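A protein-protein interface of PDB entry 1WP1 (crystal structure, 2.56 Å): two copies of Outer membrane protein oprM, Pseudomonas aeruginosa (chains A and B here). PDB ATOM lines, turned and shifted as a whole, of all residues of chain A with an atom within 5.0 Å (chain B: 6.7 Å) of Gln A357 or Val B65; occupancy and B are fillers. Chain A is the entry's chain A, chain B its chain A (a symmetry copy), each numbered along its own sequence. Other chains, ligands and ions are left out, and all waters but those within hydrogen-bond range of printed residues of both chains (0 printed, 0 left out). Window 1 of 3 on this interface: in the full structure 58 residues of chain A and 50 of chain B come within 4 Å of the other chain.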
ATOM      1  N   ALA A 278     -19.805   5.604 -23.534  1.00  0.00           N
ATOM      2  CA  ALA A 278     -20.449   4.552 -22.776  1.00  0.00           C
ATOM      3  C   ALA A 278     -19.552   3.311 -22.663  1.00  0.00           C
ATOM      4  O   ALA A 278     -19.510   2.705 -21.605  1.00  0.00           O
ATOM      5  CB  ALA A 278     -21.852   4.214 -23.349  1.00  0.00           C
ATOM      6  N   ILE A 353     -24.941  -3.240 -15.421  1.00  0.00           N
ATOM      7  CA  ILE A 353     -25.564  -1.947 -15.645  1.00  0.00           C
ATOM      8  C   ILE A 353     -24.906  -1.238 -16.824  1.00  0.00           C
ATOM      9  O   ILE A 353     -25.612  -0.762 -17.710  1.00  0.00           O
ATOM     10  CB  ILE A 353     -25.556  -1.048 -14.370  1.00  0.00           C
ATOM     11  CG1 ILE A 353     -26.421  -1.687 -13.272  1.00  0.00           C
ATOM     12  CG2 ILE A 353     -25.999   0.396 -14.713  1.00  0.00           C
ATOM     13  CD1 ILE A 353     -26.355  -0.957 -11.903  1.00  0.00           C
ATOM     14  N   ASN A 354     -23.574  -1.212 -16.877  1.00  0.00           N
ATOM     15  CA  ASN A 354     -22.898  -0.511 -17.984  1.00  0.00           C
ATOM     16  C   ASN A 354     -22.969  -1.219 -19.320  1.00  0.00           C
ATOM     17  O   ASN A 354     -22.907  -0.557 -20.352  1.00  0.00           O
ATOM     18  CB  ASN A 354     -21.450  -0.183 -17.659  1.00  0.00           C
ATOM     19  CG  ASN A 354     -21.320   0.986 -16.717  1.00  0.00           C
ATOM     20  OD1 ASN A 354     -21.157   2.108 -17.144  1.00  0.00           O
ATOM     21  ND2 ASN A 354     -21.400   0.725 -15.432  1.00  0.00           N
ATOM     22  N   VAL A 355     -23.092  -2.551 -19.317  1.00  0.00           N
ATOM     23  CA  VAL A 355     -23.386  -3.276 -20.562  1.00  0.00           C
ATOM     24  C   VAL A 355     -24.663  -2.692 -21.122  1.00  0.00           C
ATOM     25  O   VAL A 355     -24.719  -2.326 -22.297  1.00  0.00           O
ATOM     26  CB  VAL A 355     -23.547  -4.831 -20.365  1.00  0.00           C
ATOM     27  CG1 VAL A 355     -24.194  -5.486 -21.574  1.00  0.00           C
ATOM     28  CG2 VAL A 355     -22.212  -5.476 -20.089  1.00  0.00           C
ATOM     29  N   ALA A 356     -25.671  -2.572 -20.254  1.00  0.00           N
ATOM     30  CA  ALA A 356     -27.021  -2.190 -20.666  1.00  0.00           C
ATOM     31  C   ALA A 356     -27.085  -0.725 -21.093  1.00  0.00           C
ATOM     32  O   ALA A 356     -27.786  -0.379 -22.048  1.00  0.00           O
ATOM     33  CB  ALA A 356     -28.012  -2.489 -19.567  1.00  0.00           C
ATOM     34  N   GLN A 357     -26.346   0.140 -20.407  1.00  0.00           N
ATOM     35  CA  GLN A 357     -26.310   1.534 -20.826  1.00  0.00           C
ATOM     36  C   GLN A 357     -25.597   1.638 -22.171  1.00  0.00           C
ATOM     37  O   GLN A 357     -25.973   2.447 -23.006  1.00  0.00           O
ATOM     38  CB  GLN A 357     -25.655   2.426 -19.780  1.00  0.00           C
ATOM     39  CG  GLN A 357     -26.403   2.425 -18.439  1.00  0.00           C
ATOM     40  CD  GLN A 357     -25.636   3.116 -17.294  1.00  0.00           C
ATOM     41  OE1 GLN A 357     -26.242   3.794 -16.455  1.00  0.00           O
ATOM     42  NE2 GLN A 357     -24.303   2.967 -17.273  1.00  0.00           N
ATOM     43  N   TYR A 358     -24.603   0.783 -22.403  1.00  0.00           N
ATOM     44  CA  TYR A 358     -23.872   0.813 -23.655  1.00  0.00           C
ATOM     45  C   TYR A 358     -24.814   0.362 -24.763  1.00  0.00           C
ATOM     46  O   TYR A 358     -24.800   0.914 -25.855  1.00  0.00           O
ATOM     47  CB  TYR A 358     -22.614  -0.063 -23.586  1.00  0.00           C
ATOM     48  CG  TYR A 358     -21.831  -0.197 -24.886  1.00  0.00           C
ATOM     49  CD1 TYR A 358     -21.082   0.874 -25.387  1.00  0.00           C
ATOM     50  CD2 TYR A 358     -21.804  -1.417 -25.599  1.00  0.00           C
ATOM     51  CE1 TYR A 358     -20.343   0.753 -26.593  1.00  0.00           C
ATOM     52  CE2 TYR A 358     -21.069  -1.552 -26.797  1.00  0.00           C
ATOM     53  CZ  TYR A 358     -20.336  -0.458 -27.283  1.00  0.00           C
ATOM     54  OH  TYR A 358     -19.608  -0.545 -28.457  1.00  0.00           O
ATOM     55  N   GLU A 359     -25.656  -0.619 -24.474  1.00  0.00           N
ATOM     56  CA  GLU A 359     -26.543  -1.110 -25.499  1.00  0.00           C
ATOM     57  C   GLU A 359     -27.536  -0.012 -25.856  1.00  0.00           C
ATOM     58  O   GLU A 359     -27.802   0.262 -27.047  1.00  0.00           O
ATOM     59  CB  GLU A 359     -27.231  -2.383 -25.037  1.00  0.00           C
ATOM     60  CG  GLU A 359     -26.298  -3.566 -25.109  1.00  0.00           C
ATOM     61  CD  GLU A 359     -26.749  -4.755 -24.289  1.00  0.00           C
ATOM     62  OE1 GLU A 359     -27.471  -4.609 -23.285  1.00  0.00           O
ATOM     63  OE2 GLU A 359     -26.356  -5.872 -24.643  1.00  0.00           O
ATOM     64  N   LYS A 360     -28.028   0.638 -24.805  1.00  0.00           N
ATOM     65  CA  LYS A 360     -28.997   1.692 -24.919  1.00  0.00           C
ATOM     66  C   LYS A 360     -28.522   2.806 -25.828  1.00  0.00           C
ATOM     67  O   LYS A 360     -29.226   3.191 -26.778  1.00  0.00           O
ATOM     68  CB  LYS A 360     -29.278   2.234 -23.535  1.00  0.00           C
ATOM     69  CG  LYS A 360     -29.998   3.483 -23.490  1.00  0.00           C
ATOM     70  CD  LYS A 360     -31.488   3.337 -23.779  1.00  0.00           C
ATOM     71  CE  LYS A 360     -32.173   4.625 -23.169  1.00  0.00           C
ATOM     72  NZ  LYS A 360     -33.464   4.981 -23.772  1.00  0.00           N
ATOM     73  N   ALA A 361     -27.334   3.327 -25.524  1.00  0.00           N
ATOM     74  CA  ALA A 361     -26.707   4.357 -26.336  1.00  0.00           C
ATOM     75  C   ALA A 361     -26.699   3.919 -27.793  1.00  0.00           C
ATOM     76  O   ALA A 361     -26.990   4.714 -28.672  1.00  0.00           O
ATOM     77  CB  ALA A 361     -25.306   4.650 -25.856  1.00  0.00           C
ATOM     78  N   ASN B  60     -35.969  -4.064 -22.991  1.00  0.00           N
ATOM     79  CA  ASN B  60     -35.717  -2.639 -22.782  1.00  0.00           C
ATOM     80  C   ASN B  60     -34.601  -2.358 -21.767  1.00  0.00           C
ATOM     81  O   ASN B  60     -34.731  -2.661 -20.574  1.00  0.00           O
ATOM     82  CB  ASN B  60     -37.000  -1.922 -22.344  1.00  0.00           C
ATOM     83  CG  ASN B  60     -36.764  -0.444 -22.025  1.00  0.00           C
ATOM     84  OD1 ASN B  60     -36.266  -0.098 -20.948  1.00  0.00           O
ATOM     85  ND2 ASN B  60     -37.113   0.428 -22.966  1.00  0.00           N
ATOM     86  N   ARG B  61     -33.531  -1.730 -22.245  1.00  0.00           N
ATOM     87  CA  ARG B  61     -32.337  -1.502 -21.445  1.00  0.00           C
ATOM     88  C   ARG B  61     -32.511  -0.610 -20.203  1.00  0.00           C
ATOM     89  O   ARG B  61     -31.829  -0.825 -19.212  1.00  0.00           O
ATOM     90  CB  ARG B  61     -31.165  -1.033 -22.315  1.00  0.00           C
ATOM     91  CG  ARG B  61     -30.856  -1.958 -23.541  1.00  0.00           C
ATOM     92  CD  ARG B  61     -30.453  -3.385 -23.195  1.00  0.00           C
ATOM     93  NE  ARG B  61     -31.191  -4.313 -24.038  1.00  0.00           N
ATOM     94  CZ  ARG B  61     -30.675  -5.162 -24.918  1.00  0.00           C
ATOM     95  NH1 ARG B  61     -29.372  -5.274 -25.109  1.00  0.00           N
ATOM     96  NH2 ARG B  61     -31.490  -5.928 -25.608  1.00  0.00           N
ATOM     97  N   ASP B  62     -33.424   0.356 -20.240  1.00  0.00           N
ATOM     98  CA  ASP B  62     -33.708   1.190 -19.060  1.00  0.00           C
ATOM     99  C   ASP B  62     -34.357   0.433 -17.908  1.00  0.00           C
ATOM    100  O   ASP B  62     -34.018   0.662 -16.737  1.00  0.00           O
ATOM    101  CB  ASP B  62     -34.592   2.388 -19.421  1.00  0.00           C
ATOM    102  CG  ASP B  62     -33.818   3.480 -20.123  1.00  0.00           C
ATOM    103  OD1 ASP B  62     -32.657   3.783 -19.712  1.00  0.00           O
ATOM    104  OD2 ASP B  62     -34.361   4.057 -21.086  1.00  0.00           O
ATOM    105  N   LEU B  63     -35.311  -0.434 -18.235  1.00  0.00           N
ATOM    106  CA  LEU B  63     -35.901  -1.257 -17.226  1.00  0.00           C
ATOM    107  C   LEU B  63     -34.857  -2.280 -16.734  1.00  0.00           C
ATOM    108  O   LEU B  63     -34.790  -2.585 -15.540  1.00  0.00           O
ATOM    109  CB  LEU B  63     -37.157  -1.925 -17.756  1.00  0.00           C
ATOM    110  CG  LEU B  63     -37.912  -2.805 -16.750  1.00  0.00           C
ATOM    111  CD1 LEU B  63     -38.520  -1.965 -15.624  1.00  0.00           C
ATOM    112  CD2 LEU B  63     -38.992  -3.613 -17.456  1.00  0.00           C
ATOM    113  N   ARG B  64     -34.019  -2.774 -17.638  1.00  0.00           N
ATOM    114  CA  ARG B  64     -32.977  -3.711 -17.255  1.00  0.00           C
ATOM    115  C   ARG B  64     -32.008  -3.057 -16.235  1.00  0.00           C
ATOM    116  O   ARG B  64     -31.579  -3.686 -15.256  1.00  0.00           O
ATOM    117  CB  ARG B  64     -32.251  -4.199 -18.509  1.00  0.00           C
ATOM    118  CG  ARG B  64     -31.156  -5.254 -18.266  1.00  0.00           C
ATOM    119  CD  ARG B  64     -30.760  -5.950 -19.578  1.00  0.00           C
ATOM    120  NE  ARG B  64     -31.851  -6.762 -20.119  1.00  0.00           N
ATOM    121  CZ  ARG B  64     -31.823  -7.337 -21.317  1.00  0.00           C
ATOM    122  NH1 ARG B  64     -30.766  -7.180 -22.099  1.00  0.00           N
ATOM    123  NH2 ARG B  64     -32.849  -8.071 -21.743  1.00  0.00           N
ATOM    124  N   VAL B  65     -31.678  -1.791 -16.461  1.00  0.00           N
ATOM    125  CA  VAL B  65     -30.871  -1.030 -15.518  1.00  0.00           C
ATOM    126  C   VAL B  65     -31.597  -0.957 -14.178  1.00  0.00           C
ATOM    127  O   VAL B  65     -31.000  -1.194 -13.125  1.00  0.00           O
ATOM    128  CB  VAL B  65     -30.502   0.398 -16.041  1.00  0.00           C
ATOM    129  CG1 VAL B  65     -29.911   1.254 -14.908  1.00  0.00           C
ATOM    130  CG2 VAL B  65     -29.513   0.333 -17.252  1.00  0.00           C
ATOM    131  N   ALA B  66     -32.890  -0.662 -14.208  1.00  0.00           N
ATOM    132  CA  ALA B  66     -33.641  -0.582 -12.957  1.00  0.00           C
ATOM    133  C   ALA B  66     -33.614  -1.896 -12.126  1.00  0.00           C
ATOM    134  O   ALA B  66     -33.484  -1.848 -10.896  1.00  0.00           O
ATOM    135  CB  ALA B  66     -35.040  -0.123 -13.214  1.00  0.00           C
ATOM    136  N   ALA B  67     -33.733  -3.050 -12.783  1.00  0.00           N
ATOM    137  CA  ALA B  67     -33.666  -4.327 -12.078  1.00  0.00           C
ATOM    138  C   ALA B  67     -32.264  -4.572 -11.544  1.00  0.00           C
ATOM    139  O   ALA B  67     -32.093  -4.981 -10.399  1.00  0.00           O
ATOM    140  CB  ALA B  67     -34.099  -5.480 -12.972  1.00  0.00           C
ATOM    141  N   LEU B  68     -31.250  -4.316 -12.365  1.00  0.00           N
ATOM    142  CA  LEU B  68     -29.866  -4.464 -11.915  1.00  0.00           C
ATOM    143  C   LEU B  68     -29.588  -3.620 -10.657  1.00  0.00           C
ATOM    144  O   LEU B  68     -28.909  -4.064  -9.739  1.00  0.00           O
ATOM    145  CB  LEU B  68     -28.892  -4.127 -13.049  1.00  0.00           C
ATOM    146  CG  LEU B  68     -28.803  -5.231 -14.122  1.00  0.00           C
ATOM    147  CD1 LEU B  68     -28.086  -4.743 -15.381  1.00  0.00           C
ATOM    148  CD2 LEU B  68     -28.164  -6.508 -13.582  1.00  0.00           C
ATOM    149  N   ASN B  69     -30.172  -2.434 -10.606  1.00  0.00           N
ATOM    150  CA  ASN B  69     -29.999  -1.538  -9.492  1.00  0.00           C
ATOM    151  C   ASN B  69     -30.589  -2.066  -8.202  1.00  0.00           C
ATOM    152  O   ASN B  69     -30.057  -1.834  -7.124  1.00  0.00           O
ATOM    153  CB  ASN B  69     -30.627  -0.200  -9.819  1.00  0.00           C
ATOM    154  CG  ASN B  69     -29.859   0.923  -9.244  1.00  0.00           C
ATOM    155  OD1 ASN B  69     -28.612   0.923  -9.257  1.00  0.00           O
ATOM    156  ND2 ASN B  69     -30.576   1.897  -8.693  1.00  0.00           N
ATOM    157  N   VAL B  70     -31.701  -2.772  -8.307  1.00  0.00           N
ATOM    158  CA  VAL B  70     -32.222  -3.484  -7.167  1.00  0.00           C
ATOM    159  C   VAL B  70     -31.159  -4.445  -6.614  1.00  0.00           C
ATOM    160  O   VAL B  70     -30.931  -4.495  -5.411  1.00  0.00           O
ATOM    161  CB  VAL B  70     -33.491  -4.246  -7.540  1.00  0.00           C
ATOM    162  CG1 VAL B  70     -33.897  -5.218  -6.430  1.00  0.00           C
ATOM    163  CG2 VAL B  70     -34.599  -3.245  -7.854  1.00  0.00           C
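OE1 of Glu A359 lies within salt-bridge range of NH1 of Arg B61 (2.7 Å).
NZ of Lys A360 is in salt-bridge range of OD2 of Asp B62, at 3.0 Å.
The side-chain amide nitrogen (NE2) of Gln A357 lies within hydrogen-bond range of the side-chain amide oxygen (OD1) of Asn A354, 3.3 Å away.
The side-chain amide oxygen (OD1) of Asn B60 lies within hydrogen-bond range of the backbone NH (N) of Asp B62 (3.0 Å).
CG1 of Ile A353 touches CB of Leu B68, at 3.5 Å.
Ile A353 touches Asn B69.
Ala A356 touches Arg B61 (O to CB, 3.5 Å).
CG2 of Val B65 touches CB of Ala A356 (3.9 Å).
CG of Gln A357 touches CG2 of Val B65, 3.9 Å away.
Lys A360 touches Arg B61 (CB to CB, 3.97 Å).
Of the printed residues of chain B, Ile A353 touches Leu B68 and Asn B69.
Printed residues of chain B within 4 Å of Ala A356: Arg B61 and Val B65.
Gln A357 touches just one residue of chain B: Val B65.
Of the printed residues of chain B, Lys A360 touches Arg B61 (3.97 Å) and Asp B62 (3.0 Å).
Printed residues of chain A within 4 Å of Val B65: Ala A356 (3.9 Å) and Gln A357 (3.9 Å).
Of the printed residues of chain A, Leu B68 touches Ile A353.
Of the printed residues of chain A, Asn B69 touches Ile A353 (3.95 Å).
The nearest residue of chain B that does not touch Gln A357 is Arg B61 (5.3 Å).
The nearest printed residue of chain A that does not touch Val B65 is Ile A353 (4.01 Å).
Hydrophobic or aromatic side chains of chain B within 4 Å of the printed part of chain A: Val B65 and Leu B68.
Among the printed residues, Asp or Glu carboxylates within 4 Å of a Lys or Arg side-chain nitrogen of the other chain: Glu A359 with Arg B61 and Lys A360 with Asp B62.
No position is printed for both chains.
Of the 8 pairs that touch across the chains among the printed residues, none has its exchanged pair printed and touching as well.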
